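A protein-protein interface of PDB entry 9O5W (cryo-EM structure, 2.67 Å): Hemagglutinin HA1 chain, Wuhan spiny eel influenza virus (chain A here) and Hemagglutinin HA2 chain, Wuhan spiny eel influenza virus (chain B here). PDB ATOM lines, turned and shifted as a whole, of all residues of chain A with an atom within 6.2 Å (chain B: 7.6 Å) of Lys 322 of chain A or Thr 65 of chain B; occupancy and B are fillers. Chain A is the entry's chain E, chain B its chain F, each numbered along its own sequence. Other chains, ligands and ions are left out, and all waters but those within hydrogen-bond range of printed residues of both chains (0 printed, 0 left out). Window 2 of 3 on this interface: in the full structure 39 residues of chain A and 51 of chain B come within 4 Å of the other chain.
Pro 307 of chain A touches Asn 62 of chain B. O of Pro 307 of chain A touches CG2 of Thr 65 of chain B, 3.4 Å away. Phe 308 of chain A touches Met 61 of chain B (CZ to O, 3.7 Å). Phe 308 of chain A touches Thr 65 of chain B. Ile 102 of chain B touches Phe 308 of chain A (CG2 to CZ, 3.5 Å). O of Thr 65 of chain B touches CE of Lys 322 of chain A (3.4 Å). Trp 323 of chain A touches Ala 99 of chain B. Val 324 of chain A touches Ile 102 of chain B.
Of the 13 printed residues of chain A, 6 touch a printed residue of chain B. Printed residues of chain A that touch a printed residue of chain B: Lys 304, Pro 307, Phe 308, Lys 322, Trp 323 and Val 324. Hydrophobic or aromatic side chains of chain A within 4 Å of the printed part of chain B: Pro 307, Phe 308 and Val 324. Of the 14 printed residues of chain B, 5 touch a printed residue of chain A. Hydrophobic or aromatic side chains of chain B that line the printed part of chain A: Ala 99 and Ile 102. Among the printed residues, no Asp or Glu carboxylate lies within 4 Å of a Lys or Arg side-chain nitrogen of the other chain.
The side-chain amino group of Lys 304 of chain A sits at hydrogen-bond distance from the side-chain hydroxyl of Thr 65 of chain B.
N of Val 324 of chain A lies within hydrogen-bond range of O of Tyr 309 of chain A (3.1 Å). The backbone carbonyl oxygen (O) of Pro 307 of chain A is in hydrogen-bond range of the backbone NH (N) of Lys 322 of chain A (3.0 Å). O of Asn 62 of chain B lies within hydrogen-bond range of OG1 of Thr 65 of chain B, 3.2 Å away. N of Tyr 309 of chain A lies within hydrogen-bond range of O of Lys 322 of chain A, 3.0 Å away. The backbone carbonyl oxygen (O) of Phe 308 of chain A is in hydrogen-bond range of the side-chain hydroxyl (OG1) of Thr 306 of chain A (2.7 Å). NZ of Lys 304 of chain A lies within hydrogen-bond range of OD1 of Asn 319 of chain A, at 3.1 Å.
Of the printed residues of chain B, Lys 304 of chain A touches Thr 65 (3.0 Å). Of the printed residues of chain B, Phe 308 of chain A touches Met 61 (3.7 Å), Thr 65 (3.7 Å) and Ile 102 (3.5 Å). Lys 322 of chain A touches one residue of chain B. Of the printed residues of chain A, Met 61 of chain B touches Phe 308 (3.7 Å). Of the printed residues of chain A, Asn 62 of chain B touches Pro 307. Of chain A, only Lys 304 (3.0 Å), Pro 307 (3.4 Å), Phe 308 (3.7 Å) and Lys 322 (3.4 Å) come within 4 Å of Thr 65 of chain B. Ala 95 of chain B touches none of the printed residues of chain A. Of the printed residues of chain A, Ala 99 of chain B touches Trp 323 (3.5 Å). The nearest residue of chain B that does not touch Lys 322 of chain A is Ile 102 of chain B (4.1 Å).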
ATOM      1  N   LYS A 304      -2.430   0.195 -11.114  1.00  0.00           N
ATOM      2  CA  LYS A 304      -3.303  -0.931 -11.434  1.00  0.00           C
ATOM      3  C   LYS A 304      -4.344  -0.469 -12.449  1.00  0.00           C
ATOM      4  O   LYS A 304      -5.531  -0.329 -12.123  1.00  0.00           O
ATOM      5  CB  LYS A 304      -3.957  -1.480 -10.168  1.00  0.00           C
ATOM      6  CG  LYS A 304      -4.806  -2.726 -10.364  1.00  0.00           C
ATOM      7  CD  LYS A 304      -5.422  -3.161  -9.047  1.00  0.00           C
ATOM      8  CE  LYS A 304      -6.302  -4.383  -9.214  1.00  0.00           C
ATOM      9  NZ  LYS A 304      -6.982  -4.748  -7.944  1.00  0.00           N
ATOM     10  N   THR A 306      -5.541  -2.114 -14.884  1.00  0.00           N
ATOM     11  CA  THR A 306      -6.394  -3.261 -15.142  1.00  0.00           C
ATOM     12  C   THR A 306      -6.196  -4.189 -13.954  1.00  0.00           C
ATOM     13  O   THR A 306      -5.193  -4.078 -13.240  1.00  0.00           O
ATOM     14  CB  THR A 306      -6.062  -3.971 -16.465  1.00  0.00           C
ATOM     15  OG1 THR A 306      -4.844  -4.698 -16.327  1.00  0.00           O
ATOM     16  CG2 THR A 306      -5.919  -2.976 -17.613  1.00  0.00           C
ATOM     17  N   PRO A 307      -7.125  -5.117 -13.714  1.00  0.00           N
ATOM     18  CA  PRO A 307      -6.946  -6.041 -12.582  1.00  0.00           C
ATOM     19  C   PRO A 307      -5.829  -7.056 -12.736  1.00  0.00           C
ATOM     20  O   PRO A 307      -5.399  -7.602 -11.715  1.00  0.00           O
ATOM     21  CB  PRO A 307      -8.302  -6.748 -12.493  1.00  0.00           C
ATOM     22  CG  PRO A 307      -8.838  -6.663 -13.844  1.00  0.00           C
ATOM     23  CD  PRO A 307      -8.414  -5.350 -14.390  1.00  0.00           C
ATOM     24  N   PHE A 308      -5.345  -7.329 -13.947  1.00  0.00           N
ATOM     25  CA  PHE A 308      -4.353  -8.374 -14.162  1.00  0.00           C
ATOM     26  C   PHE A 308      -3.165  -7.809 -14.924  1.00  0.00           C
ATOM     27  O   PHE A 308      -3.272  -6.769 -15.575  1.00  0.00           O
ATOM     28  CB  PHE A 308      -4.991  -9.521 -14.952  1.00  0.00           C
ATOM     29  CG  PHE A 308      -6.285 -10.001 -14.359  1.00  0.00           C
ATOM     30  CD1 PHE A 308      -6.381 -10.327 -13.019  1.00  0.00           C
ATOM     31  CD2 PHE A 308      -7.420 -10.084 -15.144  1.00  0.00           C
ATOM     32  CE1 PHE A 308      -7.581 -10.746 -12.480  1.00  0.00           C
ATOM     33  CE2 PHE A 308      -8.621 -10.498 -14.609  1.00  0.00           C
ATOM     34  CZ  PHE A 308      -8.701 -10.831 -13.276  1.00  0.00           C
ATOM     35  N   TYR A 309      -2.006  -8.459 -14.784  1.00  0.00           N
ATOM     36  CA  TYR A 309      -0.813  -8.054 -15.516  1.00  0.00           C
ATOM     37  C   TYR A 309      -0.127  -9.280 -16.104  1.00  0.00           C
ATOM     38  O   TYR A 309      -0.277 -10.402 -15.614  1.00  0.00           O
ATOM     39  CB  TYR A 309       0.168  -7.257 -14.638  1.00  0.00           C
ATOM     40  CG  TYR A 309       0.959  -8.036 -13.608  1.00  0.00           C
ATOM     41  CD1 TYR A 309       0.422  -8.350 -12.373  1.00  0.00           C
ATOM     42  CD2 TYR A 309       2.262  -8.439 -13.875  1.00  0.00           C
ATOM     43  CE1 TYR A 309       1.152  -9.052 -11.438  1.00  0.00           C
ATOM     44  CE2 TYR A 309       2.994  -9.144 -12.948  1.00  0.00           C
ATOM     45  CZ  TYR A 309       2.440  -9.439 -11.728  1.00  0.00           C
ATOM     46  OH  TYR A 309       3.169 -10.140 -10.798  1.00  0.00           O
ATOM     47  N   THR A 310       0.641  -9.040 -17.167  1.00  0.00           N
ATOM     48  CA  THR A 310       1.424 -10.056 -17.874  1.00  0.00           C
ATOM     49  C   THR A 310       2.882  -9.613 -17.901  1.00  0.00           C
ATOM     50  O   THR A 310       3.288  -8.828 -18.764  1.00  0.00           O
ATOM     51  CB  THR A 310       0.892 -10.300 -19.284  1.00  0.00           C
ATOM     52  OG1 THR A 310       0.824  -9.067 -20.013  1.00  0.00           O
ATOM     53  CG2 THR A 310      -0.468 -10.963 -19.235  1.00  0.00           C
ATOM     54  N   GLY A 318      -0.156  -4.197  -1.460  1.00  0.00           N
ATOM     55  CA  GLY A 318      -1.093  -3.126  -1.736  1.00  0.00           C
ATOM     56  C   GLY A 318      -2.135  -3.521  -2.764  1.00  0.00           C
ATOM     57  O   GLY A 318      -2.455  -4.696  -2.958  1.00  0.00           O
ATOM     58  N   ASN A 319      -2.680  -2.503  -3.436  1.00  0.00           N
ATOM     59  CA  ASN A 319      -3.777  -2.702  -4.383  1.00  0.00           C
ATOM     60  C   ASN A 319      -3.117  -3.108  -5.694  1.00  0.00           C
ATOM     61  O   ASN A 319      -2.981  -2.327  -6.639  1.00  0.00           O
ATOM     62  CB  ASN A 319      -4.608  -1.434  -4.526  1.00  0.00           C
ATOM     63  CG  ASN A 319      -5.855  -1.643  -5.353  1.00  0.00           C
ATOM     64  OD1 ASN A 319      -6.245  -2.775  -5.636  1.00  0.00           O
ATOM     65  ND2 ASN A 319      -6.489  -0.548  -5.748  1.00  0.00           N
ATOM     66  N   CYS A 320      -2.710  -4.355  -5.732  1.00  0.00           N
ATOM     67  CA  CYS A 320      -1.891  -4.885  -6.800  1.00  0.00           C
ATOM     68  C   CYS A 320      -2.706  -5.659  -7.834  1.00  0.00           C
ATOM     69  O   CYS A 320      -3.723  -6.271  -7.496  1.00  0.00           O
ATOM     70  CB  CYS A 320      -0.850  -5.824  -6.195  1.00  0.00           C
ATOM     71  SG  CYS A 320       0.212  -4.994  -5.014  1.00  0.00           S
ATOM     72  N   PRO A 321      -2.293  -5.663  -9.103  1.00  0.00           N
ATOM     73  CA  PRO A 321      -2.895  -6.587 -10.067  1.00  0.00           C
ATOM     74  C   PRO A 321      -2.369  -7.995  -9.830  1.00  0.00           C
ATOM     75  O   PRO A 321      -1.286  -8.187  -9.274  1.00  0.00           O
ATOM     76  CB  PRO A 321      -2.453  -6.027 -11.420  1.00  0.00           C
ATOM     77  CG  PRO A 321      -1.176  -5.354 -11.135  1.00  0.00           C
ATOM     78  CD  PRO A 321      -1.285  -4.801  -9.752  1.00  0.00           C
ATOM     79  N   LYS A 322      -3.145  -8.989 -10.260  1.00  0.00           N
ATOM     80  CA  LYS A 322      -2.698 -10.375 -10.172  1.00  0.00           C
ATOM     81  C   LYS A 322      -2.037 -10.824 -11.465  1.00  0.00           C
ATOM     82  O   LYS A 322      -2.428 -10.432 -12.565  1.00  0.00           O
ATOM     83  CB  LYS A 322      -3.866 -11.311  -9.863  1.00  0.00           C
ATOM     84  CG  LYS A 322      -4.513 -11.110  -8.512  1.00  0.00           C
ATOM     85  CD  LYS A 322      -3.594 -11.518  -7.375  1.00  0.00           C
ATOM     86  CE  LYS A 322      -4.300 -11.446  -6.037  1.00  0.00           C
ATOM     87  NZ  LYS A 322      -3.404 -11.832  -4.915  1.00  0.00           N
ATOM     88  N   TRP A 323      -1.024 -11.668 -11.311  1.00  0.00           N
ATOM     89  CA  TRP A 323      -0.322 -12.222 -12.456  1.00  0.00           C
ATOM     90  C   TRP A 323      -1.154 -13.275 -13.178  1.00  0.00           C
ATOM     91  O   TRP A 323      -1.766 -14.148 -12.558  1.00  0.00           O
ATOM     92  CB  TRP A 323       1.010 -12.797 -11.976  1.00  0.00           C
ATOM     93  CG  TRP A 323       1.872 -13.367 -13.031  1.00  0.00           C
ATOM     94  CD1 TRP A 323       2.796 -12.708 -13.780  1.00  0.00           C
ATOM     95  CD2 TRP A 323       1.939 -14.738 -13.424  1.00  0.00           C
ATOM     96  NE1 TRP A 323       3.421 -13.580 -14.634  1.00  0.00           N
ATOM     97  CE2 TRP A 323       2.911 -14.835 -14.434  1.00  0.00           C
ATOM     98  CE3 TRP A 323       1.260 -15.894 -13.026  1.00  0.00           C
ATOM     99  CZ2 TRP A 323       3.220 -16.038 -15.055  1.00  0.00           C
ATOM    100  CZ3 TRP A 323       1.566 -17.084 -13.645  1.00  0.00           C
ATOM    101  CH2 TRP A 323       2.538 -17.149 -14.646  1.00  0.00           C
ATOM    102  N   VAL A 324      -1.162 -13.178 -14.511  1.00  0.00           N
ATOM    103  CA  VAL A 324      -1.765 -14.154 -15.407  1.00  0.00           C
ATOM    104  C   VAL A 324      -0.722 -14.518 -16.458  1.00  0.00           C
ATOM    105  O   VAL A 324       0.269 -13.810 -16.646  1.00  0.00           O
ATOM    106  CB  VAL A 324      -3.079 -13.649 -16.051  1.00  0.00           C
ATOM    107  CG1 VAL A 324      -4.115 -13.366 -14.976  1.00  0.00           C
ATOM    108  CG2 VAL A 324      -2.861 -12.403 -16.893  1.00  0.00           C
ATOM    109  N   ASN B  60     -17.186  -8.308 -11.383  1.00  0.00           N
ATOM    110  CA  ASN B  60     -17.108  -9.507 -10.563  1.00  0.00           C
ATOM    111  C   ASN B  60     -15.807 -10.245 -10.814  1.00  0.00           C
ATOM    112  O   ASN B  60     -15.515 -11.227 -10.125  1.00  0.00           O
ATOM    113  CB  ASN B  60     -18.296 -10.433 -10.819  1.00  0.00           C
ATOM    114  CG  ASN B  60     -19.562  -9.951 -10.147  1.00  0.00           C
ATOM    115  OD1 ASN B  60     -19.710 -10.070  -8.930  1.00  0.00           O
ATOM    116  ND2 ASN B  60     -20.473  -9.389 -10.926  1.00  0.00           N
ATOM    117  N   MET B  61     -15.018  -9.777 -11.783  1.00  0.00           N
ATOM    118  CA  MET B  61     -13.707 -10.306 -12.095  1.00  0.00           C
ATOM    119  C   MET B  61     -12.645  -9.512 -11.346  1.00  0.00           C
ATOM    120  O   MET B  61     -11.557 -10.032 -11.079  1.00  0.00           O
ATOM    121  CB  MET B  61     -13.519 -10.322 -13.613  1.00  0.00           C
ATOM    122  CG  MET B  61     -14.210 -11.567 -14.180  1.00  0.00           C
ATOM    123  SD  MET B  61     -14.471 -11.775 -15.953  1.00  0.00           S
ATOM    124  CE  MET B  61     -13.171 -10.813 -16.671  1.00  0.00           C
ATOM    125  N   ASN B  62     -12.956  -8.253 -11.004  1.00  0.00           N
ATOM    126  CA  ASN B  62     -12.055  -7.393 -10.249  1.00  0.00           C
ATOM    127  C   ASN B  62     -11.952  -7.807  -8.787  1.00  0.00           C
ATOM    128  O   ASN B  62     -11.072  -7.294  -8.086  1.00  0.00           O
ATOM    129  CB  ASN B  62     -12.516  -5.933 -10.301  1.00  0.00           C
ATOM    130  CG  ASN B  62     -12.353  -5.311 -11.670  1.00  0.00           C
ATOM    131  OD1 ASN B  62     -11.653  -5.839 -12.528  1.00  0.00           O
ATOM    132  ND2 ASN B  62     -12.983  -4.161 -11.870  1.00  0.00           N
ATOM    133  N   LYS B  63     -12.813  -8.713  -8.310  1.00  0.00           N
ATOM    134  CA  LYS B  63     -12.757  -9.164  -6.926  1.00  0.00           C
ATOM    135  C   LYS B  63     -11.809 -10.333  -6.735  1.00  0.00           C
ATOM    136  O   LYS B  63     -11.524 -10.690  -5.588  1.00  0.00           O
ATOM    137  CB  LYS B  63     -14.128  -9.556  -6.348  1.00  0.00           C
ATOM    138  CG  LYS B  63     -15.111  -8.411  -6.135  1.00  0.00           C
ATOM    139  CD  LYS B  63     -16.461  -8.937  -5.612  1.00  0.00           C
ATOM    140  CE  LYS B  63     -17.584  -8.917  -6.618  1.00  0.00           C
ATOM    141  NZ  LYS B  63     -18.431  -7.698  -6.514  1.00  0.00           N
ATOM    142  N   MET B  64     -11.309 -10.938  -7.811  1.00  0.00           N
ATOM    143  CA  MET B  64     -10.455 -12.102  -7.644  1.00  0.00           C
ATOM    144  C   MET B  64      -9.028 -11.699  -7.314  1.00  0.00           C
ATOM    145  O   MET B  64      -8.178 -12.576  -7.129  1.00  0.00           O
ATOM    146  CB  MET B  64     -10.466 -12.966  -8.903  1.00  0.00           C
ATOM    147  CG  MET B  64     -11.803 -13.604  -9.191  1.00  0.00           C
ATOM    148  SD  MET B  64     -11.777 -14.572 -10.702  1.00  0.00           S
ATOM    149  CE  MET B  64     -10.892 -16.028 -10.160  1.00  0.00           C
ATOM    150  N   THR B  65      -8.751 -10.394  -7.248  1.00  0.00           N
ATOM    151  CA  THR B  65      -7.444  -9.869  -6.904  1.00  0.00           C
ATOM    152  C   THR B  65      -7.409  -9.434  -5.443  1.00  0.00           C
ATOM    153  O   THR B  65      -6.360  -8.989  -4.965  1.00  0.00           O
ATOM    154  CB  THR B  65      -7.090  -8.670  -7.798  1.00  0.00           C
ATOM    155  OG1 THR B  65      -7.941  -7.565  -7.471  1.00  0.00           O
ATOM    156  CG2 THR B  65      -7.272  -8.992  -9.285  1.00  0.00           C
ATOM    157  N   GLU B  66      -8.541  -9.550  -4.732  1.00  0.00           N
ATOM    158  CA  GLU B  66      -8.716  -9.097  -3.359  1.00  0.00           C
ATOM    159  C   GLU B  66      -9.061 -10.254  -2.423  1.00  0.00           C
ATOM    160  O   GLU B  66      -9.820 -10.065  -1.471  1.00  0.00           O
ATOM    161  CB  GLU B  66      -9.797  -8.019  -3.285  1.00  0.00           C
ATOM    162  CG  GLU B  66      -9.483  -6.746  -4.090  1.00  0.00           C
ATOM    163  CD  GLU B  66     -10.698  -6.105  -4.757  1.00  0.00           C
ATOM    164  OE1 GLU B  66     -11.820  -6.649  -4.679  1.00  0.00           O
ATOM    165  OE2 GLU B  66     -10.524  -5.033  -5.371  1.00  0.00           O
ATOM    166  N   ARG B  67      -8.515 -11.449  -2.660  1.00  0.00           N
ATOM    167  CA  ARG B  67      -8.864 -12.607  -1.844  1.00  0.00           C
ATOM    168  C   ARG B  67      -7.943 -12.807  -0.647  1.00  0.00           C
ATOM    169  O   ARG B  67      -8.063 -13.829   0.035  1.00  0.00           O
ATOM    170  CB  ARG B  67      -8.907 -13.896  -2.670  1.00  0.00           C
ATOM    171  CG  ARG B  67     -10.000 -13.939  -3.718  1.00  0.00           C
ATOM    172  CD  ARG B  67     -10.034 -15.300  -4.388  1.00  0.00           C
ATOM    173  NE  ARG B  67     -11.139 -15.425  -5.333  1.00  0.00           N
ATOM    174  CZ  ARG B  67     -11.396 -16.508  -6.056  1.00  0.00           C
ATOM    175  NH1 ARG B  67     -10.645 -17.595  -5.974  1.00  0.00           N
ATOM    176  NH2 ARG B  67     -12.442 -16.504  -6.877  1.00  0.00           N
ATOM    177  N   ALA B  68      -7.042 -11.872  -0.370  1.00  0.00           N
ATOM    178  CA  ALA B  68      -6.183 -11.966   0.802  1.00  0.00           C
ATOM    179  C   ALA B  68      -6.905 -11.220   1.916  1.00  0.00           C
ATOM    180  O   ALA B  68      -7.093 -10.001   1.829  1.00  0.00           O
ATOM    181  CB  ALA B  68      -4.805 -11.367   0.533  1.00  0.00           C
ATOM    182  N   ARG B  94      -0.328 -20.731  -4.892  1.00  0.00           N
ATOM    183  CA  ARG B  94      -1.460 -19.814  -4.866  1.00  0.00           C
ATOM    184  C   ARG B  94      -1.516 -18.990  -6.148  1.00  0.00           C
ATOM    185  O   ARG B  94      -2.587 -18.830  -6.747  1.00  0.00           O
ATOM    186  CB  ARG B  94      -1.371 -18.909  -3.637  1.00  0.00           C
ATOM    187  CG  ARG B  94      -2.587 -18.023  -3.425  1.00  0.00           C
ATOM    188  CD  ARG B  94      -2.439 -17.161  -2.190  1.00  0.00           C
ATOM    189  NE  ARG B  94      -3.696 -16.512  -1.834  1.00  0.00           N
ATOM    190  CZ  ARG B  94      -3.865 -15.700  -0.799  1.00  0.00           C
ATOM    191  NH1 ARG B  94      -2.862 -15.366  -0.001  1.00  0.00           N
ATOM    192  NH2 ARG B  94      -5.076 -15.204  -0.557  1.00  0.00           N
ATOM    193  N   ALA B  95      -0.364 -18.487  -6.606  1.00  0.00           N
ATOM    194  CA  ALA B  95      -0.340 -17.674  -7.817  1.00  0.00           C
ATOM    195  C   ALA B  95      -0.723 -18.478  -9.054  1.00  0.00           C
ATOM    196  O   ALA B  95      -1.464 -17.984  -9.914  1.00  0.00           O
ATOM    197  CB  ALA B  95       1.044 -17.055  -7.998  1.00  0.00           C
ATOM    198  N   THR B  98      -4.495 -19.205  -8.951  1.00  0.00           N
ATOM    199  CA  THR B  98      -5.241 -17.984  -9.211  1.00  0.00           C
ATOM    200  C   THR B  98      -5.213 -17.651 -10.697  1.00  0.00           C
ATOM    201  O   THR B  98      -6.242 -17.272 -11.267  1.00  0.00           O
ATOM    202  CB  THR B  98      -4.670 -16.842  -8.364  1.00  0.00           C
ATOM    203  OG1 THR B  98      -4.811 -17.166  -6.977  1.00  0.00           O
ATOM    204  CG2 THR B  98      -5.397 -15.523  -8.623  1.00  0.00           C
ATOM    205  N   ALA B  99      -4.045 -17.758 -11.340  1.00  0.00           N
ATOM    206  CA  ALA B  99      -3.975 -17.456 -12.767  1.00  0.00           C
ATOM    207  C   ALA B  99      -4.861 -18.399 -13.576  1.00  0.00           C
ATOM    208  O   ALA B  99      -5.548 -17.969 -14.517  1.00  0.00           O
ATOM    209  CB  ALA B  99      -2.526 -17.539 -13.245  1.00  0.00           C
ATOM    210  N   ILE B 102      -8.433 -17.349 -13.178  1.00  0.00           N
ATOM    211  CA  ILE B 102      -8.719 -16.120 -13.908  1.00  0.00           C
ATOM    212  C   ILE B 102      -8.954 -16.452 -15.380  1.00  0.00           C
ATOM    213  O   ILE B 102      -9.857 -15.903 -16.025  1.00  0.00           O
ATOM    214  CB  ILE B 102      -7.579 -15.103 -13.697  1.00  0.00           C
ATOM    215  CG1 ILE B 102      -7.566 -14.626 -12.239  1.00  0.00           C
ATOM    216  CG2 ILE B 102      -7.743 -13.877 -14.611  1.00  0.00           C
ATOM    217  CD1 ILE B 102      -6.283 -13.919 -11.810  1.00  0.00           C
